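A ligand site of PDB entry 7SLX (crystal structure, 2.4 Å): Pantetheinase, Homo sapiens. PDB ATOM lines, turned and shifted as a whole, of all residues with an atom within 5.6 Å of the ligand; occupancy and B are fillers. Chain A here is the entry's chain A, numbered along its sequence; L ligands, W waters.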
ATOM      1  N   GLU A  78       1.047 -24.749 -21.021  1.00  0.00           N
ATOM      2  CA  GLU A  78       0.924 -23.382 -20.559  1.00  0.00           C
ATOM      3  C   GLU A  78       1.834 -23.239 -19.324  1.00  0.00           C
ATOM      4  O   GLU A  78       1.872 -24.158 -18.504  1.00  0.00           O
ATOM      5  CB  GLU A  78      -0.517 -23.127 -20.136  1.00  0.00           C
ATOM      6  CG  GLU A  78      -0.732 -21.739 -19.587  1.00  0.00           C
ATOM      7  CD  GLU A  78      -2.066 -21.543 -18.898  1.00  0.00           C
ATOM      8  OE1 GLU A  78      -2.663 -22.543 -18.449  1.00  0.00           O
ATOM      9  OE2 GLU A  78      -2.502 -20.373 -18.802  1.00  0.00           O
ATOM     10  N   ASP A  79       2.543 -22.101 -19.199  1.00  0.00           N
ATOM     11  CA  ASP A  79       3.422 -21.798 -18.059  1.00  0.00           C
ATOM     12  C   ASP A  79       4.589 -22.778 -17.872  1.00  0.00           C
ATOM     13  O   ASP A  79       5.180 -22.802 -16.800  1.00  0.00           O
ATOM     14  CB  ASP A  79       2.618 -21.700 -16.742  1.00  0.00           C
ATOM     15  CG  ASP A  79       1.590 -20.586 -16.692  1.00  0.00           C
ATOM     16  OD1 ASP A  79       1.808 -19.543 -17.350  1.00  0.00           O
ATOM     17  OD2 ASP A  79       0.568 -20.757 -15.985  1.00  0.00           O
ATOM     18  N   TRP A  84       3.297 -20.546 -12.682  1.00  0.00           N
ATOM     19  CA  TRP A  84       2.062 -19.795 -12.489  1.00  0.00           C
ATOM     20  C   TRP A  84       2.033 -18.911 -11.224  1.00  0.00           C
ATOM     21  O   TRP A  84       0.975 -18.355 -10.898  1.00  0.00           O
ATOM     22  CB  TRP A  84       0.866 -20.775 -12.484  1.00  0.00           C
ATOM     23  CG  TRP A  84       1.138 -21.995 -11.634  1.00  0.00           C
ATOM     24  CD1 TRP A  84       0.906 -22.126 -10.296  1.00  0.00           C
ATOM     25  CD2 TRP A  84       1.834 -23.176 -12.049  1.00  0.00           C
ATOM     26  NE1 TRP A  84       1.404 -23.328  -9.855  1.00  0.00           N
ATOM     27  CE2 TRP A  84       1.970 -23.995 -10.908  1.00  0.00           C
ATOM     28  CE3 TRP A  84       2.369 -23.610 -13.270  1.00  0.00           C
ATOM     29  CZ2 TRP A  84       2.591 -25.251 -10.967  1.00  0.00           C
ATOM     30  CZ3 TRP A  84       3.005 -24.841 -13.323  1.00  0.00           C
ATOM     31  CH2 TRP A  84       3.098 -25.655 -12.190  1.00  0.00           C
ATOM     32  N   LYS A 177      -4.116 -15.062 -24.168  1.00  0.00           N
ATOM     33  CA  LYS A 177      -5.222 -15.670 -23.426  1.00  0.00           C
ATOM     34  C   LYS A 177      -6.347 -14.678 -23.095  1.00  0.00           C
ATOM     35  O   LYS A 177      -6.119 -13.596 -22.518  1.00  0.00           O
ATOM     36  CB  LYS A 177      -4.709 -16.404 -22.170  1.00  0.00           C
ATOM     37  CG  LYS A 177      -5.719 -17.295 -21.463  1.00  0.00           C
ATOM     38  CD  LYS A 177      -5.057 -17.949 -20.243  1.00  0.00           C
ATOM     39  CE  LYS A 177      -5.949 -19.002 -19.596  1.00  0.00           C
ATOM     40  NZ  LYS A 177      -5.397 -19.490 -18.320  1.00  0.00           N
ATOM     41  N   ASN A 179      -9.505 -15.692 -21.549  1.00  0.00           N
ATOM     42  CA  ASN A 179     -10.199 -16.020 -20.320  1.00  0.00           C
ATOM     43  C   ASN A 179      -9.274 -16.332 -19.173  1.00  0.00           C
ATOM     44  O   ASN A 179      -9.010 -17.481 -18.857  1.00  0.00           O
ATOM     45  CB  ASN A 179     -11.213 -17.136 -20.551  1.00  0.00           C
ATOM     46  CG  ASN A 179     -12.183 -16.752 -21.636  1.00  0.00           C
ATOM     47  OD1 ASN A 179     -13.132 -16.006 -21.387  1.00  0.00           O
ATOM     48  ND2 ASN A 179     -11.953 -17.180 -22.875  1.00  0.00           N
ATOM     49  N   PHE A 181      -8.018 -16.859 -15.429  1.00  0.00           N
ATOM     50  CA  PHE A 181      -8.562 -17.518 -14.253  1.00  0.00           C
ATOM     51  C   PHE A 181      -8.249 -16.655 -13.039  1.00  0.00           C
ATOM     52  O   PHE A 181      -7.384 -15.788 -13.117  1.00  0.00           O
ATOM     53  CB  PHE A 181      -7.893 -18.884 -14.099  1.00  0.00           C
ATOM     54  CG  PHE A 181      -8.446 -19.744 -12.984  1.00  0.00           C
ATOM     55  CD1 PHE A 181      -9.729 -20.263 -13.067  1.00  0.00           C
ATOM     56  CD2 PHE A 181      -7.672 -20.039 -11.878  1.00  0.00           C
ATOM     57  CE1 PHE A 181     -10.217 -21.105 -12.054  1.00  0.00           C
ATOM     58  CE2 PHE A 181      -8.162 -20.864 -10.851  1.00  0.00           C
ATOM     59  CZ  PHE A 181      -9.435 -21.396 -10.952  1.00  0.00           C
ATOM     60  N   GLU A 184      -4.790 -14.650 -11.822  1.00  0.00           N
ATOM     61  CA  GLU A 184      -3.883 -14.452 -12.951  1.00  0.00           C
ATOM     62  C   GLU A 184      -3.797 -12.946 -13.111  1.00  0.00           C
ATOM     63  O   GLU A 184      -4.008 -12.410 -14.209  1.00  0.00           O
ATOM     64  CB  GLU A 184      -4.335 -15.154 -14.227  1.00  0.00           C
ATOM     65  CG  GLU A 184      -3.822 -16.565 -14.378  1.00  0.00           C
ATOM     66  CD  GLU A 184      -4.069 -17.192 -15.734  1.00  0.00           C
ATOM     67  OE1 GLU A 184      -5.235 -17.196 -16.189  1.00  0.00           O
ATOM     68  OE2 GLU A 184      -3.107 -17.734 -16.327  1.00  0.00           O
ATOM     69  N   CSO A 210      -5.886 -23.317 -21.873  1.00  0.00           N
ATOM     70  CA  CSO A 210      -6.532 -23.697 -20.600  1.00  0.00           C
ATOM     71  CB  CSO A 210      -5.613 -23.126 -19.544  1.00  0.00           C
ATOM     72  SG  CSO A 210      -5.813 -24.105 -18.047  1.00  0.00           S
ATOM     73  C   CSO A 210      -8.025 -23.341 -20.408  1.00  0.00           C
ATOM     74  O   CSO A 210      -8.875 -23.953 -21.027  1.00  0.00           O
ATOM     75  OD  CSO A 210      -5.040 -22.929 -17.377  1.00  0.00           O
ATOM     76  N   PHE A 211      -8.319 -22.398 -19.509  1.00  0.00           N
ATOM     77  CA  PHE A 211      -9.666 -21.928 -19.140  1.00  0.00           C
ATOM     78  C   PHE A 211     -10.503 -21.490 -20.325  1.00  0.00           C
ATOM     79  O   PHE A 211     -11.735 -21.479 -20.223  1.00  0.00           O
ATOM     80  CB  PHE A 211      -9.523 -20.769 -18.139  1.00  0.00           C
ATOM     81  CG  PHE A 211     -10.669 -20.606 -17.165  1.00  0.00           C
ATOM     82  CD1 PHE A 211     -11.408 -21.705 -16.740  1.00  0.00           C
ATOM     83  CD2 PHE A 211     -10.950 -19.364 -16.606  1.00  0.00           C
ATOM     84  CE1 PHE A 211     -12.429 -21.558 -15.804  1.00  0.00           C
ATOM     85  CE2 PHE A 211     -11.978 -19.221 -15.665  1.00  0.00           C
ATOM     86  CZ  PHE A 211     -12.697 -20.324 -15.253  1.00  0.00           C
ATOM     87  N   LEU A 214     -13.664 -23.406 -21.564  1.00  0.00           N
ATOM     88  CA  LEU A 214     -14.964 -23.278 -20.878  1.00  0.00           C
ATOM     89  C   LEU A 214     -15.825 -22.146 -21.388  1.00  0.00           C
ATOM     90  O   LEU A 214     -16.957 -22.008 -20.935  1.00  0.00           O
ATOM     91  CB  LEU A 214     -14.787 -23.177 -19.349  1.00  0.00           C
ATOM     92  CG  LEU A 214     -14.649 -24.520 -18.684  1.00  0.00           C
ATOM     93  CD1 LEU A 214     -14.098 -24.386 -17.287  1.00  0.00           C
ATOM     94  CD2 LEU A 214     -15.959 -25.326 -18.754  1.00  0.00           C
ATOM     95  N   ALA A 236      -2.440 -25.848 -18.110  1.00  0.00           N
ATOM     96  CA  ALA A 236      -1.892 -26.015 -16.743  1.00  0.00           C
ATOM     97  C   ALA A 236      -3.123 -26.240 -15.865  1.00  0.00           C
ATOM     98  O   ALA A 236      -3.449 -25.413 -15.035  1.00  0.00           O
ATOM     99  CB  ALA A 236      -1.164 -24.738 -16.317  1.00  0.00           C
ATOM    100  N   TRP A 237      -3.848 -27.330 -16.129  1.00  0.00           N
ATOM    101  CA  TRP A 237      -5.171 -27.684 -15.590  1.00  0.00           C
ATOM    102  C   TRP A 237      -5.185 -28.386 -14.220  1.00  0.00           C
ATOM    103  O   TRP A 237      -4.556 -29.424 -14.020  1.00  0.00           O
ATOM    104  CB  TRP A 237      -5.898 -28.542 -16.638  1.00  0.00           C
ATOM    105  CG  TRP A 237      -7.357 -28.765 -16.424  1.00  0.00           C
ATOM    106  CD1 TRP A 237      -7.944 -29.775 -15.706  1.00  0.00           C
ATOM    107  CD2 TRP A 237      -8.429 -28.073 -17.093  1.00  0.00           C
ATOM    108  NE1 TRP A 237      -9.312 -29.735 -15.860  1.00  0.00           N
ATOM    109  CE2 TRP A 237      -9.633 -28.688 -16.699  1.00  0.00           C
ATOM    110  CE3 TRP A 237      -8.486 -26.982 -17.970  1.00  0.00           C
ATOM    111  CZ2 TRP A 237     -10.885 -28.264 -17.166  1.00  0.00           C
ATOM    112  CZ3 TRP A 237      -9.732 -26.517 -18.380  1.00  0.00           C
ATOM    113  CH2 TRP A 237     -10.914 -27.160 -17.997  1.00  0.00           C
ATOM    114  N   MET A 238      -6.009 -27.849 -13.314  1.00  0.00           N
ATOM    115  CA  MET A 238      -6.212 -28.451 -12.000  1.00  0.00           C
ATOM    116  C   MET A 238      -7.411 -29.358 -12.128  1.00  0.00           C
ATOM    117  O   MET A 238      -8.514 -28.897 -12.423  1.00  0.00           O
ATOM    118  CB  MET A 238      -6.460 -27.380 -10.938  1.00  0.00           C
ATOM    119  CG  MET A 238      -5.242 -26.581 -10.604  1.00  0.00           C
ATOM    120  SD  MET A 238      -5.635 -25.305  -9.361  1.00  0.00           S
ATOM    121  CE  MET A 238      -6.613 -24.187 -10.292  1.00  0.00           C
ATOM    122  N   ASN A 239      -7.201 -30.641 -11.948  1.00  0.00           N
ATOM    123  CA  ASN A 239      -8.261 -31.635 -12.088  1.00  0.00           C
ATOM    124  C   ASN A 239      -9.347 -31.505 -11.049  1.00  0.00           C
ATOM    125  O   ASN A 239      -9.054 -31.310  -9.870  1.00  0.00           O
ATOM    126  CB  ASN A 239      -7.673 -33.040 -12.071  1.00  0.00           C
ATOM    127  CG  ASN A 239      -6.837 -33.354 -13.275  1.00  0.00           C
ATOM    128  OD1 ASN A 239      -7.092 -32.872 -14.394  1.00  0.00           O
ATOM    129  ND2 ASN A 239      -5.892 -34.283 -13.111  1.00  0.00           N
ATOM    130  N   VAL A 240     -10.612 -31.527 -11.500  1.00  0.00           N
ATOM    131  CA  VAL A 240     -11.787 -31.491 -10.625  1.00  0.00           C
ATOM    132  C   VAL A 240     -12.779 -32.572 -11.029  1.00  0.00           C
ATOM    133  O   VAL A 240     -13.553 -32.375 -11.932  1.00  0.00           O
ATOM    134  CB  VAL A 240     -12.470 -30.095 -10.435  1.00  0.00           C
ATOM    135  CG1 VAL A 240     -13.617 -30.179  -9.429  1.00  0.00           C
ATOM    136  CG2 VAL A 240     -11.476 -29.040 -10.004  1.00  0.00           C
ATOM    137  N   LEU A 244     -14.591 -32.498 -14.459  1.00  0.00           N
ATOM    138  CA  LEU A 244     -13.585 -31.602 -14.960  1.00  0.00           C
ATOM    139  C   LEU A 244     -12.164 -32.084 -14.769  1.00  0.00           C
ATOM    140  O   LEU A 244     -11.249 -31.287 -14.507  1.00  0.00           O
ATOM    141  CB  LEU A 244     -13.841 -30.199 -14.401  1.00  0.00           C
ATOM    142  CG  LEU A 244     -15.107 -29.562 -15.051  1.00  0.00           C
ATOM    143  CD1 LEU A 244     -15.539 -28.315 -14.340  1.00  0.00           C
ATOM    144  CD2 LEU A 244     -14.939 -29.363 -16.553  1.00  0.00           C
ATOM    145  N   LYS A 271      -0.813 -30.361  -7.166  1.00  0.00           N
ATOM    146  CA  LYS A 271      -1.870 -29.386  -7.462  1.00  0.00           C
ATOM    147  C   LYS A 271      -2.935 -30.021  -8.329  1.00  0.00           C
ATOM    148  O   LYS A 271      -3.812 -29.338  -8.856  1.00  0.00           O
ATOM    149  CB  LYS A 271      -1.296 -28.136  -8.148  1.00  0.00           C
ATOM    150  CG  LYS A 271      -0.769 -27.101  -7.171  1.00  0.00           C
ATOM    151  CD  LYS A 271      -0.356 -25.792  -7.872  1.00  0.00           C
ATOM    152  CE  LYS A 271      -1.502 -24.871  -8.237  1.00  0.00           C
ATOM    153  NZ  LYS A 271      -2.282 -24.383  -7.058  1.00  0.00           N
ATOM    154  N   MET A 273      -2.427 -31.540 -11.134  1.00  0.00           N
ATOM    155  CA  MET A 273      -2.112 -31.240 -12.522  1.00  0.00           C
ATOM    156  C   MET A 273      -1.500 -32.475 -13.203  1.00  0.00           C
ATOM    157  O   MET A 273      -0.361 -32.848 -12.918  1.00  0.00           O
ATOM    158  CB  MET A 273      -1.186 -30.003 -12.630  1.00  0.00           C
ATOM    159  CG  MET A 273      -1.775 -28.757 -11.993  1.00  0.00           C
ATOM    160  SD  MET A 273      -0.621 -27.380 -12.034  1.00  0.00           S
ATOM    161  CE  MET A 273      -1.727 -26.066 -12.184  1.00  0.00           C
ATOM    162  N   PHE A 337     -18.938 -30.084  -7.439  1.00  0.00           N
ATOM    163  CA  PHE A 337     -18.080 -28.917  -7.692  1.00  0.00           C
ATOM    164  C   PHE A 337     -18.818 -27.600  -7.345  1.00  0.00           C
ATOM    165  O   PHE A 337     -18.944 -26.682  -8.172  1.00  0.00           O
ATOM    166  CB  PHE A 337     -17.499 -28.978  -9.127  1.00  0.00           C
ATOM    167  CG  PHE A 337     -16.555 -27.876  -9.557  1.00  0.00           C
ATOM    168  CD1 PHE A 337     -15.610 -27.344  -8.669  1.00  0.00           C
ATOM    169  CD2 PHE A 337     -16.604 -27.356 -10.849  1.00  0.00           C
ATOM    170  CE1 PHE A 337     -14.763 -26.315  -9.075  1.00  0.00           C
ATOM    171  CE2 PHE A 337     -15.739 -26.339 -11.252  1.00  0.00           C
ATOM    172  CZ  PHE A 337     -14.837 -25.808 -10.356  1.00  0.00           C
ATOM    173  N   HIS A 386     -22.690 -21.592 -12.463  1.00  0.00           N
ATOM    174  CA  HIS A 386     -21.544 -21.895 -11.616  1.00  0.00           C
ATOM    175  C   HIS A 386     -20.940 -20.542 -11.290  1.00  0.00           C
ATOM    176  O   HIS A 386     -20.811 -19.699 -12.180  1.00  0.00           O
ATOM    177  CB  HIS A 386     -20.500 -22.755 -12.363  1.00  0.00           C
ATOM    178  CG  HIS A 386     -19.355 -23.155 -11.497  1.00  0.00           C
ATOM    179  ND1 HIS A 386     -19.326 -24.390 -10.918  1.00  0.00           N
ATOM    180  CD2 HIS A 386     -18.289 -22.458 -11.080  1.00  0.00           C
ATOM    181  CE1 HIS A 386     -18.232 -24.412 -10.181  1.00  0.00           C
ATOM    182  NE2 HIS A 386     -17.588 -23.266 -10.234  1.00  0.00           N
ATOM    183  N   VAL A 388     -18.392 -20.418  -8.288  1.00  0.00           N
ATOM    184  CA  VAL A 388     -17.160 -20.623  -7.511  1.00  0.00           C
ATOM    185  C   VAL A 388     -15.921 -20.690  -8.415  1.00  0.00           C
ATOM    186  O   VAL A 388     -15.726 -21.647  -9.173  1.00  0.00           O
ATOM    187  CB  VAL A 388     -17.229 -21.808  -6.513  1.00  0.00           C
ATOM    188  CG1 VAL A 388     -15.895 -22.002  -5.795  1.00  0.00           C
ATOM    189  CG2 VAL A 388     -18.373 -21.613  -5.500  1.00  0.00           C
ATOM    190  N   GLU A 389     -15.069 -19.648  -8.298  1.00  0.00           N
ATOM    191  CA  GLU A 389     -13.799 -19.451  -8.995  1.00  0.00           C
ATOM    192  C   GLU A 389     -13.974 -19.248 -10.518  1.00  0.00           C
ATOM    193  O   GLU A 389     -13.035 -19.463 -11.287  1.00  0.00           O
ATOM    194  CB  GLU A 389     -12.789 -20.568  -8.647  1.00  0.00           C
ATOM    195  CG  GLU A 389     -12.390 -20.589  -7.172  1.00  0.00           C
ATOM    196  CD  GLU A 389     -11.559 -21.775  -6.708  1.00  0.00           C
ATOM    197  OE1 GLU A 389     -10.500 -22.035  -7.324  1.00  0.00           O
ATOM    198  OE2 GLU A 389     -11.927 -22.397  -5.688  1.00  0.00           O
ATOM    199  N   TYR A 392     -20.041 -19.303 -15.251  1.00  0.00           N
ATOM    200  CA  TYR A 392     -20.478 -19.955 -16.466  1.00  0.00           C
ATOM    201  C   TYR A 392     -21.738 -20.739 -16.223  1.00  0.00           C
ATOM    202  O   TYR A 392     -21.814 -21.473 -15.229  1.00  0.00           O
ATOM    203  CB  TYR A 392     -19.361 -20.870 -17.068  1.00  0.00           C
ATOM    204  CG  TYR A 392     -18.508 -21.623 -16.071  1.00  0.00           C
ATOM    205  CD1 TYR A 392     -17.348 -21.066 -15.560  1.00  0.00           C
ATOM    206  CD2 TYR A 392     -18.791 -22.950 -15.766  1.00  0.00           C
ATOM    207  CE1 TYR A 392     -16.557 -21.758 -14.654  1.00  0.00           C
ATOM    208  CE2 TYR A 392     -17.973 -23.676 -14.893  1.00  0.00           C
ATOM    209  CZ  TYR A 392     -16.865 -23.069 -14.330  1.00  0.00           C
ATOM    210  OH  TYR A 392     -16.060 -23.755 -13.465  1.00  0.00           O
HETATM  211  N1  LIG L   1      -9.391 -26.349 -13.568  1.00  0.00           N
HETATM  212  C1  LIG L   1      -8.702 -25.244 -13.987  1.00  0.00           C
HETATM  213  N2  LIG L   1      -7.311 -25.410 -14.080  1.00  0.00           N
HETATM  214  C2  LIG L   1     -11.596 -27.568 -13.607  1.00  0.00           C
HETATM  215  C3  LIG L   1     -11.780 -26.344 -14.475  1.00  0.00           C
HETATM  216  C4  LIG L   1     -10.532 -25.779 -10.878  1.00  0.00           C
HETATM  217  C5  LIG L   1      -4.302 -20.628 -14.951  1.00  0.00           C
HETATM  218  C6  LIG L   1     -11.140 -25.495 -12.113  1.00  0.00           C
HETATM  219  N3  LIG L   1     -12.291 -23.652 -11.066  1.00  0.00           N
HETATM  220  C7  LIG L   1      -3.292 -23.076 -11.668  1.00  0.00           C
HETATM  221  C8  LIG L   1      -3.619 -22.724 -13.037  1.00  0.00           C
HETATM  222  C9  LIG L   1      -6.628 -24.317 -14.422  1.00  0.00           C
HETATM  223  C10 LIG L   1      -7.224 -23.079 -14.669  1.00  0.00           C
HETATM  224  C11 LIG L   1      -8.624 -23.024 -14.641  1.00  0.00           C
HETATM  225  N4  LIG L   1      -9.399 -24.077 -14.292  1.00  0.00           N
HETATM  226  C12 LIG L   1     -10.810 -26.300 -13.302  1.00  0.00           C
HETATM  227  N5  LIG L   1     -10.780 -25.048  -9.756  1.00  0.00           N
HETATM  228  C13 LIG L   1     -11.665 -24.022  -9.915  1.00  0.00           C
HETATM  229  C14 LIG L   1     -12.009 -24.400 -12.162  1.00  0.00           C
HETATM  230  C15 LIG L   1      -6.447 -21.910 -15.117  1.00  0.00           C
HETATM  231  O1  LIG L   1      -6.786 -21.263 -16.102  1.00  0.00           O
HETATM  232  N6  LIG L   1      -5.305 -21.554 -14.399  1.00  0.00           N
HETATM  233  C16 LIG L   1      -2.935 -21.342 -15.004  1.00  0.00           C
HETATM  234  C17 LIG L   1      -2.536 -21.799 -13.602  1.00  0.00           C
HETATM  235  C18 LIG L   1      -4.991 -22.014 -13.049  1.00  0.00           C
HETATM  236  N7  LIG L   1      -3.033 -23.359 -10.578  1.00  0.00           N
HETATM  237  O   HOH W   1     -14.488 -22.160 -11.958  1.00  0.00           O
HETATM  238  O   HOH W   2     -11.519 -25.568  -6.472  1.00  0.00           O
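An oxygen (O1) of the ligand sits at hydrogen-bond distance from OD of CSO 210, at 2.7 Å.
The backbone NH of Met 238 sits at hydrogen-bond distance from a nitrogen (N2) of the ligand (2.9 Å).
O of Met 238 is in hydrogen-bond range of N1 of the ligand, 2.9 Å away.
NZ of Lys 177 lies within hydrogen-bond range of O1 of the ligand (3.2 Å).
OD of CSO 210 is in hydrogen-bond range of the side-chain carboxylate of Glu 78.
N of Phe 181 is in hydrogen-bond range of OE1 of Glu 184 (2.9 Å).
The indole nitrogen (NE1) of Trp 237 sits at hydrogen-bond distance from the backbone carbonyl oxygen (O) of Leu 244, 2.8 Å away.
SG of CSO 210 is in hydrogen-bond range of the backbone NH (N) of Ala 236 (3.8 Å).
The side-chain amino group (NZ) of Lys 177 lies within salt-bridge range of the side-chain carboxylate (OE1) of Glu 184, 3.1 Å away.
The side-chain carboxylate (OE1) of Glu 78 lies within hydrogen-bond range of the backbone NH (N) of Ala 236, 3.3 Å away.
OE2 of Glu 78 is in salt-bridge range of NZ of Lys 177.
OE1 of Glu 78 touches C16 of the ligand, at 3.7 Å.
Asp 79 touches the ligand.
Trp 84 touches the ligand (CB to C17, 3.7 Å).
Phe 181 touches the ligand (CB to O1, 3.3 Å).
OE2 of Glu 184 touches C5 of the ligand (3.4 Å).
Phe 211 touches the ligand (CB to O1, 3.4 Å).
Ala 236 touches the ligand (O to C8, 3.4 Å).
Trp 237 touches the ligand.
Val 240 touches the ligand.
Leu 244 touches the ligand.
CE of Lys 271 touches N7 of the ligand, at 3.2 Å.
Met 273 touches the ligand.
Phe 337 touches the ligand.
OE1 of Glu 389 touches C13 of the ligand, at 3.5 Å.
Hydrophobic or aromatic side chains within 4 Å of the ligand: Trp 84, Phe 181, Phe 211, Trp 237, Met 238, Val 240, Leu 244, Met 273 and Phe 337.
Along chain A the residues within 4 Å of the ligand span positions 78 to 389.
The nearest printed residue that does not touch the ligand is Leu 214 (4.1 Å).
Water W2 lies within hydrogen-bond range of OE2 of Glu 389 (3.3 Å) and N5 of the ligand (3.4 Å).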
